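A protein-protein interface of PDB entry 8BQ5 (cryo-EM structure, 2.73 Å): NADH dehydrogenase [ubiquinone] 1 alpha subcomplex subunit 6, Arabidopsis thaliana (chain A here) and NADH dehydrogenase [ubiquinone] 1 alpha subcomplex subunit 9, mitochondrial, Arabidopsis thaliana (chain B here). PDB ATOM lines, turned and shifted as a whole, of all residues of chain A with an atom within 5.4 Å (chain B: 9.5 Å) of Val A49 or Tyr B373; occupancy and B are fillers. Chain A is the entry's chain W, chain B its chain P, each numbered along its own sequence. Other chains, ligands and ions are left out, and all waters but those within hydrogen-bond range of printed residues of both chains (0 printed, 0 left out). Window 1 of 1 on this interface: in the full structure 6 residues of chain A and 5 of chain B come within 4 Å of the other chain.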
ATOM      1  N   TYR A  44       1.183  -3.480   3.948  1.00  0.00           N
ATOM      2  CA  TYR A  44       0.803  -3.155   2.581  1.00  0.00           C
ATOM      3  C   TYR A  44       1.929  -2.516   1.777  1.00  0.00           C
ATOM      4  O   TYR A  44       1.699  -2.133   0.625  1.00  0.00           O
ATOM      5  CB  TYR A  44      -0.424  -2.232   2.567  1.00  0.00           C
ATOM      6  CG  TYR A  44      -1.670  -2.828   3.190  1.00  0.00           C
ATOM      7  CD1 TYR A  44      -1.811  -2.929   4.567  1.00  0.00           C
ATOM      8  CD2 TYR A  44      -2.705  -3.297   2.392  1.00  0.00           C
ATOM      9  CE1 TYR A  44      -2.949  -3.475   5.131  1.00  0.00           C
ATOM     10  CE2 TYR A  44      -3.844  -3.846   2.946  1.00  0.00           C
ATOM     11  CZ  TYR A  44      -3.961  -3.934   4.315  1.00  0.00           C
ATOM     12  OH  TYR A  44      -5.098  -4.480   4.864  1.00  0.00           O
ATOM     13  N   ASN A  45       3.131  -2.406   2.346  1.00  0.00           N
ATOM     14  CA  ASN A  45       4.291  -1.798   1.687  1.00  0.00           C
ATOM     15  C   ASN A  45       3.924  -0.451   1.057  1.00  0.00           C
ATOM     16  O   ASN A  45       3.973  -0.257  -0.157  1.00  0.00           O
ATOM     17  CB  ASN A  45       4.891  -2.742   0.640  1.00  0.00           C
ATOM     18  CG  ASN A  45       5.001  -4.169   1.132  1.00  0.00           C
ATOM     19  OD1 ASN A  45       5.937  -4.519   1.851  1.00  0.00           O
ATOM     20  ND2 ASN A  45       4.051  -5.007   0.735  1.00  0.00           N
ATOM     21  N   LEU A  46       3.544   0.478   1.931  1.00  0.00           N
ATOM     22  CA  LEU A  46       3.097   1.801   1.515  1.00  0.00           C
ATOM     23  C   LEU A  46       4.162   2.870   1.720  1.00  0.00           C
ATOM     24  O   LEU A  46       3.831   4.059   1.757  1.00  0.00           O
ATOM     25  CB  LEU A  46       1.821   2.187   2.265  1.00  0.00           C
ATOM     26  CG  LEU A  46       0.670   1.183   2.215  1.00  0.00           C
ATOM     27  CD1 LEU A  46      -0.259   1.369   3.408  1.00  0.00           C
ATOM     28  CD2 LEU A  46      -0.096   1.291   0.908  1.00  0.00           C
ATOM     29  N   GLN A  47       5.432   2.475   1.851  1.00  0.00           N
ATOM     30  CA  GLN A  47       6.490   3.436   2.153  1.00  0.00           C
ATOM     31  C   GLN A  47       6.630   4.482   1.054  1.00  0.00           C
ATOM     32  O   GLN A  47       6.788   5.674   1.339  1.00  0.00           O
ATOM     33  CB  GLN A  47       7.817   2.705   2.371  1.00  0.00           C
ATOM     34  CG  GLN A  47       7.995   2.091   3.759  1.00  0.00           C
ATOM     35  CD  GLN A  47       6.874   1.145   4.154  1.00  0.00           C
ATOM     36  OE1 GLN A  47       6.268   0.490   3.305  1.00  0.00           O
ATOM     37  NE2 GLN A  47       6.594   1.071   5.450  1.00  0.00           N
ATOM     38  N   ASP A  48       6.576   4.058  -0.208  1.00  0.00           N
ATOM     39  CA  ASP A  48       6.665   4.966  -1.343  1.00  0.00           C
ATOM     40  C   ASP A  48       5.297   5.301  -1.922  1.00  0.00           C
ATOM     41  O   ASP A  48       5.209   5.776  -3.059  1.00  0.00           O
ATOM     42  CB  ASP A  48       7.563   4.370  -2.428  1.00  0.00           C
ATOM     43  CG  ASP A  48       9.037   4.579  -2.144  1.00  0.00           C
ATOM     44  OD1 ASP A  48       9.608   3.792  -1.361  1.00  0.00           O
ATOM     45  OD2 ASP A  48       9.622   5.531  -2.700  1.00  0.00           O
ATOM     46  N   VAL A  49       4.228   5.067  -1.159  1.00  0.00           N
ATOM     47  CA  VAL A  49       2.865   5.194  -1.651  1.00  0.00           C
ATOM     48  C   VAL A  49       2.112   6.325  -0.965  1.00  0.00           C
ATOM     49  O   VAL A  49       1.457   7.133  -1.632  1.00  0.00           O
ATOM     50  CB  VAL A  49       2.101   3.863  -1.494  1.00  0.00           C
ATOM     51  CG1 VAL A  49       0.769   3.920  -2.223  1.00  0.00           C
ATOM     52  CG2 VAL A  49       2.948   2.709  -2.003  1.00  0.00           C
ATOM     53  N   VAL A  50       2.183   6.400   0.362  1.00  0.00           N
ATOM     54  CA  VAL A  50       1.451   7.417   1.104  1.00  0.00           C
ATOM     55  C   VAL A  50       2.155   7.673   2.431  1.00  0.00           C
ATOM     56  O   VAL A  50       2.796   6.777   2.991  1.00  0.00           O
ATOM     57  CB  VAL A  50      -0.013   6.991   1.321  1.00  0.00           C
ATOM     58  CG1 VAL A  50      -0.094   5.870   2.342  1.00  0.00           C
ATOM     59  CG2 VAL A  50      -0.867   8.177   1.731  1.00  0.00           C
ATOM     60  N   ALA A  51       2.059   8.901   2.930  1.00  0.00           N
ATOM     61  CA  ALA A  51       2.661   9.234   4.209  1.00  0.00           C
ATOM     62  C   ALA A  51       1.791   8.735   5.361  1.00  0.00           C
ATOM     63  O   ALA A  51       0.568   8.643   5.230  1.00  0.00           O
ATOM     64  CB  ALA A  51       2.859  10.741   4.328  1.00  0.00           C
ATOM     65  N   ARG A  96      -5.109  -4.709  -2.065  1.00  0.00           N
ATOM     66  CA  ARG A  96      -5.235  -4.177  -3.415  1.00  0.00           C
ATOM     67  C   ARG A  96      -4.067  -3.236  -3.651  1.00  0.00           C
ATOM     68  O   ARG A  96      -3.132  -3.193  -2.846  1.00  0.00           O
ATOM     69  CB  ARG A  96      -6.565  -3.450  -3.620  1.00  0.00           C
ATOM     70  CG  ARG A  96      -7.781  -4.347  -3.585  1.00  0.00           C
ATOM     71  CD  ARG A  96      -7.727  -5.356  -4.713  1.00  0.00           C
ATOM     72  NE  ARG A  96      -7.832  -4.743  -6.034  1.00  0.00           N
ATOM     73  CZ  ARG A  96      -8.975  -4.467  -6.647  1.00  0.00           C
ATOM     74  NH1 ARG A  96     -10.142  -4.718  -6.078  1.00  0.00           N
ATOM     75  NH2 ARG A  96      -8.945  -3.933  -7.865  1.00  0.00           N
ATOM     76  N   HIS A  97      -4.106  -2.473  -4.738  1.00  0.00           N
ATOM     77  CA  HIS A  97      -3.021  -1.535  -4.981  1.00  0.00           C
ATOM     78  C   HIS A  97      -3.337  -0.193  -4.337  1.00  0.00           C
ATOM     79  O   HIS A  97      -2.659   0.223  -3.395  1.00  0.00           O
ATOM     80  CB  HIS A  97      -2.777  -1.376  -6.483  1.00  0.00           C
ATOM     81  CG  HIS A  97      -1.657  -2.220  -7.004  1.00  0.00           C
ATOM     82  ND1 HIS A  97      -1.390  -2.356  -8.349  1.00  0.00           N
ATOM     83  CD2 HIS A  97      -0.732  -2.971  -6.360  1.00  0.00           C
ATOM     84  CE1 HIS A  97      -0.351  -3.157  -8.511  1.00  0.00           C
ATOM     85  NE2 HIS A  97       0.067  -3.544  -7.320  1.00  0.00           N
ATOM     86  N   HIS A  98      -4.404   0.464  -4.780  1.00  0.00           N
ATOM     87  CA  HIS A  98      -4.657   1.835  -4.369  1.00  0.00           C
ATOM     88  C   HIS A  98      -5.758   1.958  -3.324  1.00  0.00           C
ATOM     89  O   HIS A  98      -6.309   3.051  -3.151  1.00  0.00           O
ATOM     90  CB  HIS A  98      -4.981   2.694  -5.591  1.00  0.00           C
ATOM     91  CG  HIS A  98      -3.771   3.085  -6.379  1.00  0.00           C
ATOM     92  ND1 HIS A  98      -2.867   4.024  -5.932  1.00  0.00           N
ATOM     93  CD2 HIS A  98      -3.307   2.654  -7.574  1.00  0.00           C
ATOM     94  CE1 HIS A  98      -1.901   4.161  -6.823  1.00  0.00           C
ATOM     95  NE2 HIS A  98      -2.145   3.340  -7.829  1.00  0.00           N
ATOM     96  N   VAL A 105      -6.107   4.850  -1.188  1.00  0.00           N
ATOM     97  CA  VAL A 105      -4.815   5.231  -0.645  1.00  0.00           C
ATOM     98  C   VAL A 105      -3.900   5.663  -1.789  1.00  0.00           C
ATOM     99  O   VAL A 105      -3.916   5.093  -2.881  1.00  0.00           O
ATOM    100  CB  VAL A 105      -4.183   4.094   0.184  1.00  0.00           C
ATOM    101  CG1 VAL A 105      -3.903   2.875  -0.679  1.00  0.00           C
ATOM    102  CG2 VAL A 105      -2.920   4.563   0.858  1.00  0.00           C
ATOM    103  N   GLY A 106      -3.115   6.704  -1.534  1.00  0.00           N
ATOM    104  CA  GLY A 106      -2.151   7.191  -2.504  1.00  0.00           C
ATOM    105  C   GLY A 106      -2.749   8.099  -3.560  1.00  0.00           C
ATOM    106  O   GLY A 106      -2.365   8.041  -4.729  1.00  0.00           O
ATOM    107  N   TYR B  83      -1.332  -7.847 -19.885  1.00  0.00           N
ATOM    108  CA  TYR B  83      -1.898  -6.594 -19.391  1.00  0.00           C
ATOM    109  C   TYR B  83      -2.829  -5.966 -20.417  1.00  0.00           C
ATOM    110  O   TYR B  83      -3.808  -5.305 -20.052  1.00  0.00           O
ATOM    111  CB  TYR B  83      -0.777  -5.631 -19.008  1.00  0.00           C
ATOM    112  CG  TYR B  83       0.148  -6.204 -17.966  1.00  0.00           C
ATOM    113  CD1 TYR B  83      -0.127  -6.059 -16.615  1.00  0.00           C
ATOM    114  CD2 TYR B  83       1.286  -6.907 -18.331  1.00  0.00           C
ATOM    115  CE1 TYR B  83       0.707  -6.589 -15.658  1.00  0.00           C
ATOM    116  CE2 TYR B  83       2.126  -7.441 -17.381  1.00  0.00           C
ATOM    117  CZ  TYR B  83       1.834  -7.279 -16.046  1.00  0.00           C
ATOM    118  OH  TYR B  83       2.669  -7.808 -15.095  1.00  0.00           O
ATOM    119  N   ILE B 223       8.460  -1.970 -17.388  1.00  0.00           N
ATOM    120  CA  ILE B 223       8.737  -2.501 -16.062  1.00  0.00           C
ATOM    121  C   ILE B 223       7.484  -3.189 -15.542  1.00  0.00           C
ATOM    122  O   ILE B 223       6.388  -2.620 -15.581  1.00  0.00           O
ATOM    123  CB  ILE B 223       9.194  -1.395 -15.090  1.00  0.00           C
ATOM    124  CG1 ILE B 223      10.286  -0.544 -15.737  1.00  0.00           C
ATOM    125  CG2 ILE B 223       9.689  -1.997 -13.788  1.00  0.00           C
ATOM    126  CD1 ILE B 223      11.548  -1.313 -16.047  1.00  0.00           C
ATOM    127  N   GLY B 224       7.651  -4.414 -15.061  1.00  0.00           N
ATOM    128  CA  GLY B 224       6.532  -5.174 -14.549  1.00  0.00           C
ATOM    129  C   GLY B 224       7.013  -6.477 -13.947  1.00  0.00           C
ATOM    130  O   GLY B 224       8.215  -6.720 -13.826  1.00  0.00           O
ATOM    131  N   THR B 225       6.042  -7.315 -13.577  1.00  0.00           N
ATOM    132  CA  THR B 225       6.367  -8.578 -12.923  1.00  0.00           C
ATOM    133  C   THR B 225       7.202  -9.476 -13.829  1.00  0.00           C
ATOM    134  O   THR B 225       8.165 -10.104 -13.374  1.00  0.00           O
ATOM    135  CB  THR B 225       5.086  -9.292 -12.493  1.00  0.00           C
ATOM    136  OG1 THR B 225       4.389  -8.487 -11.534  1.00  0.00           O
ATOM    137  CG2 THR B 225       5.405 -10.644 -11.873  1.00  0.00           C
ATOM    138  N   LEU B 230      14.690  -5.974 -14.894  1.00  0.00           N
ATOM    139  CA  LEU B 230      14.869  -6.042 -13.447  1.00  0.00           C
ATOM    140  C   LEU B 230      14.950  -7.484 -12.961  1.00  0.00           C
ATOM    141  O   LEU B 230      15.700  -7.788 -12.027  1.00  0.00           O
ATOM    142  CB  LEU B 230      13.740  -5.294 -12.740  1.00  0.00           C
ATOM    143  CG  LEU B 230      13.711  -3.775 -12.927  1.00  0.00           C
ATOM    144  CD1 LEU B 230      12.685  -3.144 -12.000  1.00  0.00           C
ATOM    145  CD2 LEU B 230      15.086  -3.177 -12.689  1.00  0.00           C
ATOM    146  N   TYR B 257       6.039   1.897 -16.722  1.00  0.00           N
ATOM    147  CA  TYR B 257       5.188   0.830 -16.208  1.00  0.00           C
ATOM    148  C   TYR B 257       4.455   0.142 -17.353  1.00  0.00           C
ATOM    149  O   TYR B 257       3.945   0.799 -18.263  1.00  0.00           O
ATOM    150  CB  TYR B 257       4.188   1.406 -15.206  1.00  0.00           C
ATOM    151  CG  TYR B 257       3.468   0.400 -14.333  1.00  0.00           C
ATOM    152  CD1 TYR B 257       4.007  -0.852 -14.079  1.00  0.00           C
ATOM    153  CD2 TYR B 257       2.239   0.712 -13.766  1.00  0.00           C
ATOM    154  CE1 TYR B 257       3.343  -1.765 -13.276  1.00  0.00           C
ATOM    155  CE2 TYR B 257       1.568  -0.191 -12.967  1.00  0.00           C
ATOM    156  CZ  TYR B 257       2.122  -1.427 -12.724  1.00  0.00           C
ATOM    157  OH  TYR B 257       1.452  -2.325 -11.928  1.00  0.00           O
ATOM    158  N   VAL B 258       4.407  -1.191 -17.304  1.00  0.00           N
ATOM    159  CA  VAL B 258       3.783  -1.956 -18.382  1.00  0.00           C
ATOM    160  C   VAL B 258       2.282  -1.698 -18.442  1.00  0.00           C
ATOM    161  O   VAL B 258       1.692  -1.680 -19.530  1.00  0.00           O
ATOM    162  CB  VAL B 258       4.110  -3.457 -18.228  1.00  0.00           C
ATOM    163  CG1 VAL B 258       3.393  -4.059 -17.027  1.00  0.00           C
ATOM    164  CG2 VAL B 258       3.760  -4.209 -19.502  1.00  0.00           C
ATOM    165  N   VAL B 259       1.640  -1.492 -17.289  1.00  0.00           N
ATOM    166  CA  VAL B 259       0.202  -1.238 -17.270  1.00  0.00           C
ATOM    167  C   VAL B 259      -0.115   0.076 -17.973  1.00  0.00           C
ATOM    168  O   VAL B 259      -1.151   0.209 -18.639  1.00  0.00           O
ATOM    169  CB  VAL B 259      -0.322  -1.256 -15.821  1.00  0.00           C
ATOM    170  CG1 VAL B 259      -1.791  -0.866 -15.769  1.00  0.00           C
ATOM    171  CG2 VAL B 259      -0.112  -2.628 -15.201  1.00  0.00           C
ATOM    172  N   ASP B 260       0.771   1.068 -17.840  1.00  0.00           N
ATOM    173  CA  ASP B 260       0.565   2.341 -18.524  1.00  0.00           C
ATOM    174  C   ASP B 260       0.620   2.177 -20.038  1.00  0.00           C
ATOM    175  O   ASP B 260      -0.146   2.817 -20.766  1.00  0.00           O
ATOM    176  CB  ASP B 260       1.601   3.363 -18.062  1.00  0.00           C
ATOM    177  CG  ASP B 260       1.378   3.816 -16.635  1.00  0.00           C
ATOM    178  OD1 ASP B 260       2.333   3.750 -15.837  1.00  0.00           O
ATOM    179  OD2 ASP B 260       0.252   4.240 -16.309  1.00  0.00           O
ATOM    180  N   ILE B 296      17.351   1.276  -7.286  1.00  0.00           N
ATOM    181  CA  ILE B 296      15.981   1.066  -6.820  1.00  0.00           C
ATOM    182  C   ILE B 296      15.786  -0.371  -6.360  1.00  0.00           C
ATOM    183  O   ILE B 296      15.253  -0.625  -5.273  1.00  0.00           O
ATOM    184  CB  ILE B 296      14.972   1.441  -7.921  1.00  0.00           C
ATOM    185  CG1 ILE B 296      15.076   2.921  -8.274  1.00  0.00           C
ATOM    186  CG2 ILE B 296      13.553   1.127  -7.473  1.00  0.00           C
ATOM    187  CD1 ILE B 296      14.174   3.318  -9.418  1.00  0.00           C
ATOM    188  N   MET B 300      14.995  -2.415  -2.807  1.00  0.00           N
ATOM    189  CA  MET B 300      13.796  -3.245  -2.831  1.00  0.00           C
ATOM    190  C   MET B 300      14.108  -4.690  -2.458  1.00  0.00           C
ATOM    191  O   MET B 300      13.337  -5.328  -1.734  1.00  0.00           O
ATOM    192  CB  MET B 300      13.135  -3.175  -4.208  1.00  0.00           C
ATOM    193  CG  MET B 300      12.334  -1.902  -4.450  1.00  0.00           C
ATOM    194  SD  MET B 300      10.712  -1.819  -3.653  1.00  0.00           S
ATOM    195  CE  MET B 300      10.421  -3.521  -3.172  1.00  0.00           C
ATOM    196  N   HIS B 368       2.704   6.106 -14.264  1.00  0.00           N
ATOM    197  CA  HIS B 368       3.050   5.827 -12.877  1.00  0.00           C
ATOM    198  C   HIS B 368       4.550   5.963 -12.660  1.00  0.00           C
ATOM    199  O   HIS B 368       5.351   5.608 -13.528  1.00  0.00           O
ATOM    200  CB  HIS B 368       2.613   4.415 -12.486  1.00  0.00           C
ATOM    201  CG  HIS B 368       1.193   4.323 -12.028  1.00  0.00           C
ATOM    202  ND1 HIS B 368       0.128   4.369 -12.901  1.00  0.00           N
ATOM    203  CD2 HIS B 368       0.661   4.200 -10.790  1.00  0.00           C
ATOM    204  CE1 HIS B 368      -0.999   4.268 -12.222  1.00  0.00           C
ATOM    205  NE2 HIS B 368      -0.704   4.167 -10.938  1.00  0.00           N
ATOM    206  N   LYS B 369       4.927   6.473 -11.492  1.00  0.00           N
ATOM    207  CA  LYS B 369       6.327   6.450 -11.096  1.00  0.00           C
ATOM    208  C   LYS B 369       6.757   5.020 -10.788  1.00  0.00           C
ATOM    209  O   LYS B 369       5.956   4.188 -10.353  1.00  0.00           O
ATOM    210  CB  LYS B 369       6.560   7.346  -9.882  1.00  0.00           C
ATOM    211  CG  LYS B 369       7.878   8.104  -9.918  1.00  0.00           C
ATOM    212  CD  LYS B 369       7.910   9.216  -8.881  1.00  0.00           C
ATOM    213  CE  LYS B 369       6.835  10.256  -9.146  1.00  0.00           C
ATOM    214  NZ  LYS B 369       6.641  10.507 -10.602  1.00  0.00           N
ATOM    215  N   LEU B 370       8.037   4.734 -11.029  1.00  0.00           N
ATOM    216  CA  LEU B 370       8.526   3.367 -10.876  1.00  0.00           C
ATOM    217  C   LEU B 370       8.516   2.923  -9.419  1.00  0.00           C
ATOM    218  O   LEU B 370       8.197   1.765  -9.123  1.00  0.00           O
ATOM    219  CB  LEU B 370       9.930   3.241 -11.461  1.00  0.00           C
ATOM    220  CG  LEU B 370      10.043   3.232 -12.986  1.00  0.00           C
ATOM    221  CD1 LEU B 370      11.255   2.424 -13.404  1.00  0.00           C
ATOM    222  CD2 LEU B 370       8.783   2.676 -13.627  1.00  0.00           C
ATOM    223  N   LYS B 371       8.872   3.816  -8.499  1.00  0.00           N
ATOM    224  CA  LYS B 371       8.935   3.443  -7.094  1.00  0.00           C
ATOM    225  C   LYS B 371       7.555   3.057  -6.578  1.00  0.00           C
ATOM    226  O   LYS B 371       6.545   3.674  -6.924  1.00  0.00           O
ATOM    227  CB  LYS B 371       9.505   4.592  -6.262  1.00  0.00           C
ATOM    228  CG  LYS B 371      11.021   4.654  -6.261  1.00  0.00           C
ATOM    229  CD  LYS B 371      11.512   6.088  -6.215  1.00  0.00           C
ATOM    230  CE  LYS B 371      12.723   6.227  -5.306  1.00  0.00           C
ATOM    231  NZ  LYS B 371      12.454   5.715  -3.933  1.00  0.00           N
ATOM    232  N   GLY B 372       7.520   2.019  -5.748  1.00  0.00           N
ATOM    233  CA  GLY B 372       6.277   1.565  -5.164  1.00  0.00           C
ATOM    234  C   GLY B 372       5.664   0.374  -5.872  1.00  0.00           C
ATOM    235  O   GLY B 372       6.269  -0.699  -5.941  1.00  0.00           O
ATOM    236  N   TYR B 373       4.451   0.563  -6.400  1.00  0.00           N
ATOM    237  CA  TYR B 373       3.709  -0.557  -6.978  1.00  0.00           C
ATOM    238  C   TYR B 373       4.401  -1.167  -8.192  1.00  0.00           C
ATOM    239  O   TYR B 373       4.493  -2.406  -8.263  1.00  0.00           O
ATOM    240  CB  TYR B 373       2.280  -0.112  -7.296  1.00  0.00           C
ATOM    241  CG  TYR B 373       1.482   0.165  -6.050  1.00  0.00           C
ATOM    242  CD1 TYR B 373       1.714  -0.555  -4.889  1.00  0.00           C
ATOM    243  CD2 TYR B 373       0.528   1.171  -6.019  1.00  0.00           C
ATOM    244  CE1 TYR B 373       1.003  -0.308  -3.742  1.00  0.00           C
ATOM    245  CE2 TYR B 373      -0.188   1.430  -4.872  1.00  0.00           C
ATOM    246  CZ  TYR B 373       0.059   0.690  -3.735  1.00  0.00           C
ATOM    247  OH  TYR B 373      -0.657   0.940  -2.589  1.00  0.00           O
ATOM    248  N   PRO B 374       4.892  -0.396  -9.172  1.00  0.00           N
ATOM    249  CA  PRO B 374       5.529  -1.035 -10.336  1.00  0.00           C
ATOM    250  C   PRO B 374       6.754  -1.867  -9.997  1.00  0.00           C
ATOM    251  O   PRO B 374       7.140  -2.726 -10.798  1.00  0.00           O
ATOM    252  CB  PRO B 374       5.884   0.157 -11.234  1.00  0.00           C
ATOM    253  CG  PRO B 374       4.908   1.199 -10.859  1.00  0.00           C
ATOM    254  CD  PRO B 374       4.739   1.055  -9.382  1.00  0.00           C
ATOM    255  N   VAL B 375       7.386  -1.643  -8.843  1.00  0.00           N
ATOM    256  CA  VAL B 375       8.511  -2.471  -8.421  1.00  0.00           C
ATOM    257  C   VAL B 375       8.156  -3.388  -7.259  1.00  0.00           C
ATOM    258  O   VAL B 375       9.062  -3.877  -6.570  1.00  0.00           O
ATOM    259  CB  VAL B 375       9.739  -1.609  -8.064  1.00  0.00           C
ATOM    260  CG1 VAL B 375      10.310  -0.948  -9.313  1.00  0.00           C
ATOM    261  CG2 VAL B 375       9.383  -0.569  -7.019  1.00  0.00           C
ATOM    262  N   GLU B 376       6.865  -3.645  -7.022  1.00  0.00           N
ATOM    263  CA  GLU B 376       6.471  -4.503  -5.910  1.00  0.00           C
ATOM    264  C   GLU B 376       6.843  -5.961  -6.146  1.00  0.00           C
ATOM    265  O   GLU B 376       7.005  -6.721  -5.188  1.00  0.00           O
ATOM    266  CB  GLU B 376       4.967  -4.397  -5.653  1.00  0.00           C
ATOM    267  CG  GLU B 376       4.575  -4.743  -4.223  1.00  0.00           C
ATOM    268  CD  GLU B 376       3.207  -4.219  -3.840  1.00  0.00           C
ATOM    269  OE1 GLU B 376       2.663  -3.378  -4.583  1.00  0.00           O
ATOM    270  OE2 GLU B 376       2.679  -4.641  -2.790  1.00  0.00           O
ATOM    271  N   PHE B 377       6.981  -6.374  -7.406  1.00  0.00           N
ATOM    272  CA  PHE B 377       7.304  -7.768  -7.685  1.00  0.00           C
ATOM    273  C   PHE B 377       8.691  -8.148  -7.185  1.00  0.00           C
ATOM    274  O   PHE B 377       9.013  -9.340  -7.130  1.00  0.00           O
ATOM    275  CB  PHE B 377       7.191  -8.045  -9.184  1.00  0.00           C
ATOM    276  CG  PHE B 377       8.260  -7.388 -10.004  1.00  0.00           C
ATOM    277  CD1 PHE B 377       8.169  -6.049 -10.339  1.00  0.00           C
ATOM    278  CD2 PHE B 377       9.356  -8.110 -10.444  1.00  0.00           C
ATOM    279  CE1 PHE B 377       9.149  -5.442 -11.093  1.00  0.00           C
ATOM    280  CE2 PHE B 377      10.339  -7.507 -11.198  1.00  0.00           C
ATOM    281  CZ  PHE B 377      10.236  -6.172 -11.523  1.00  0.00           C
ATOM    282  N   LEU B 378       9.517  -7.167  -6.818  1.00  0.00           N
ATOM    283  CA  LEU B 378      10.857  -7.443  -6.320  1.00  0.00           C
ATOM    284  C   LEU B 378      10.866  -7.929  -4.875  1.00  0.00           C
ATOM    285  O   LEU B 378      11.937  -8.287  -4.373  1.00  0.00           O
ATOM    286  CB  LEU B 378      11.729  -6.193  -6.461  1.00  0.00           C
ATOM    287  CG  LEU B 378      12.113  -5.820  -7.896  1.00  0.00           C
ATOM    288  CD1 LEU B 378      12.811  -4.471  -7.946  1.00  0.00           C
ATOM    289  CD2 LEU B 378      12.989  -6.901  -8.510  1.00  0.00           C
ATOM    290  N   ILE B 379       9.713  -7.946  -4.199  1.00  0.00           N
ATOM    291  CA  ILE B 379       9.643  -8.483  -2.842  1.00  0.00           C
ATOM    292  C   ILE B 379      10.047  -9.951  -2.826  1.00  0.00           C
ATOM    293  O   ILE B 379      10.676 -10.421  -1.871  1.00  0.00           O
ATOM    294  CB  ILE B 379       8.228  -8.291  -2.254  1.00  0.00           C
ATOM    295  CG1 ILE B 379       7.808  -6.821  -2.289  1.00  0.00           C
ATOM    296  CG2 ILE B 379       8.161  -8.816  -0.829  1.00  0.00           C
ATOM    297  CD1 ILE B 379       8.542  -5.946  -1.331  1.00  0.00           C
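O of His A97 sits close to OH of Tyr B373 (2.3 Å).
The side-chain amino group (NZ) of Lys B371 lies within salt-bridge range of the side-chain carboxylate (OD2) of Asp A48, 3.1 Å away.
The backbone NH (N) of Val A105 sits at hydrogen-bond distance from the backbone carbonyl oxygen (O) of His A98.
N of His B368 sits at hydrogen-bond distance from OD1 of Asp B260.
OE2 of Glu B376 touches ND2 of Asn A45, at 3.8 Å.
Leu A46 touches Tyr B373 (CD2 to OH, 3.6 Å).
Tyr B373 touches Val A49.
His A97 touches Tyr B257.
His A97 touches Glu B376 (NE2 to OE1, 3.8 Å).
His B368 touches His A98 (NE2 to NE2, 3.5 Å).
His A98 touches Tyr B373.
Of the printed residues of chain B, Leu A46 touches Tyr B373 (3.6 Å).
Of the printed residues of chain B, Asp A48 touches Lys B371.
Val A49 touches just one residue of chain B: Tyr B373.
No residue of chain B comes within 4 Å of Val A50.
No residue of chain B comes within 4 Å of Gly A106.
Of the printed residues of chain A, Tyr B257 touches His A97.
Printed residues of chain A within 4 Å of His B368: His A98.
Tyr B373 touches four residues of chain A.
Of the printed residues of chain A, Glu B376 touches Asn A45 and His A97.
Ile B379 touches none of the printed residues of chain A.
The nearest residue of chain B that does not touch Val A49 is Gly B372 (4.7 Å).
The nearest residue of chain A that does not touch Tyr B373 is Val A105 (4.2 Å).
Of the 13 printed residues of chain A, 6 touch a printed residue of chain B.
Hydrophobic or aromatic side chains of chain A within 4 Å of the printed part of chain B: Leu A46, Val A49, His A97 and His A98.
Hydrophobic or aromatic side chains of chain B within 4 Å of the printed part of chain A: Tyr B257, His B368 and Tyr B373.
Among the printed residues, Asp or Glu carboxylates within 4 Å of a Lys or Arg side-chain nitrogen of the other chain: Asp A48 with Lys B371.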
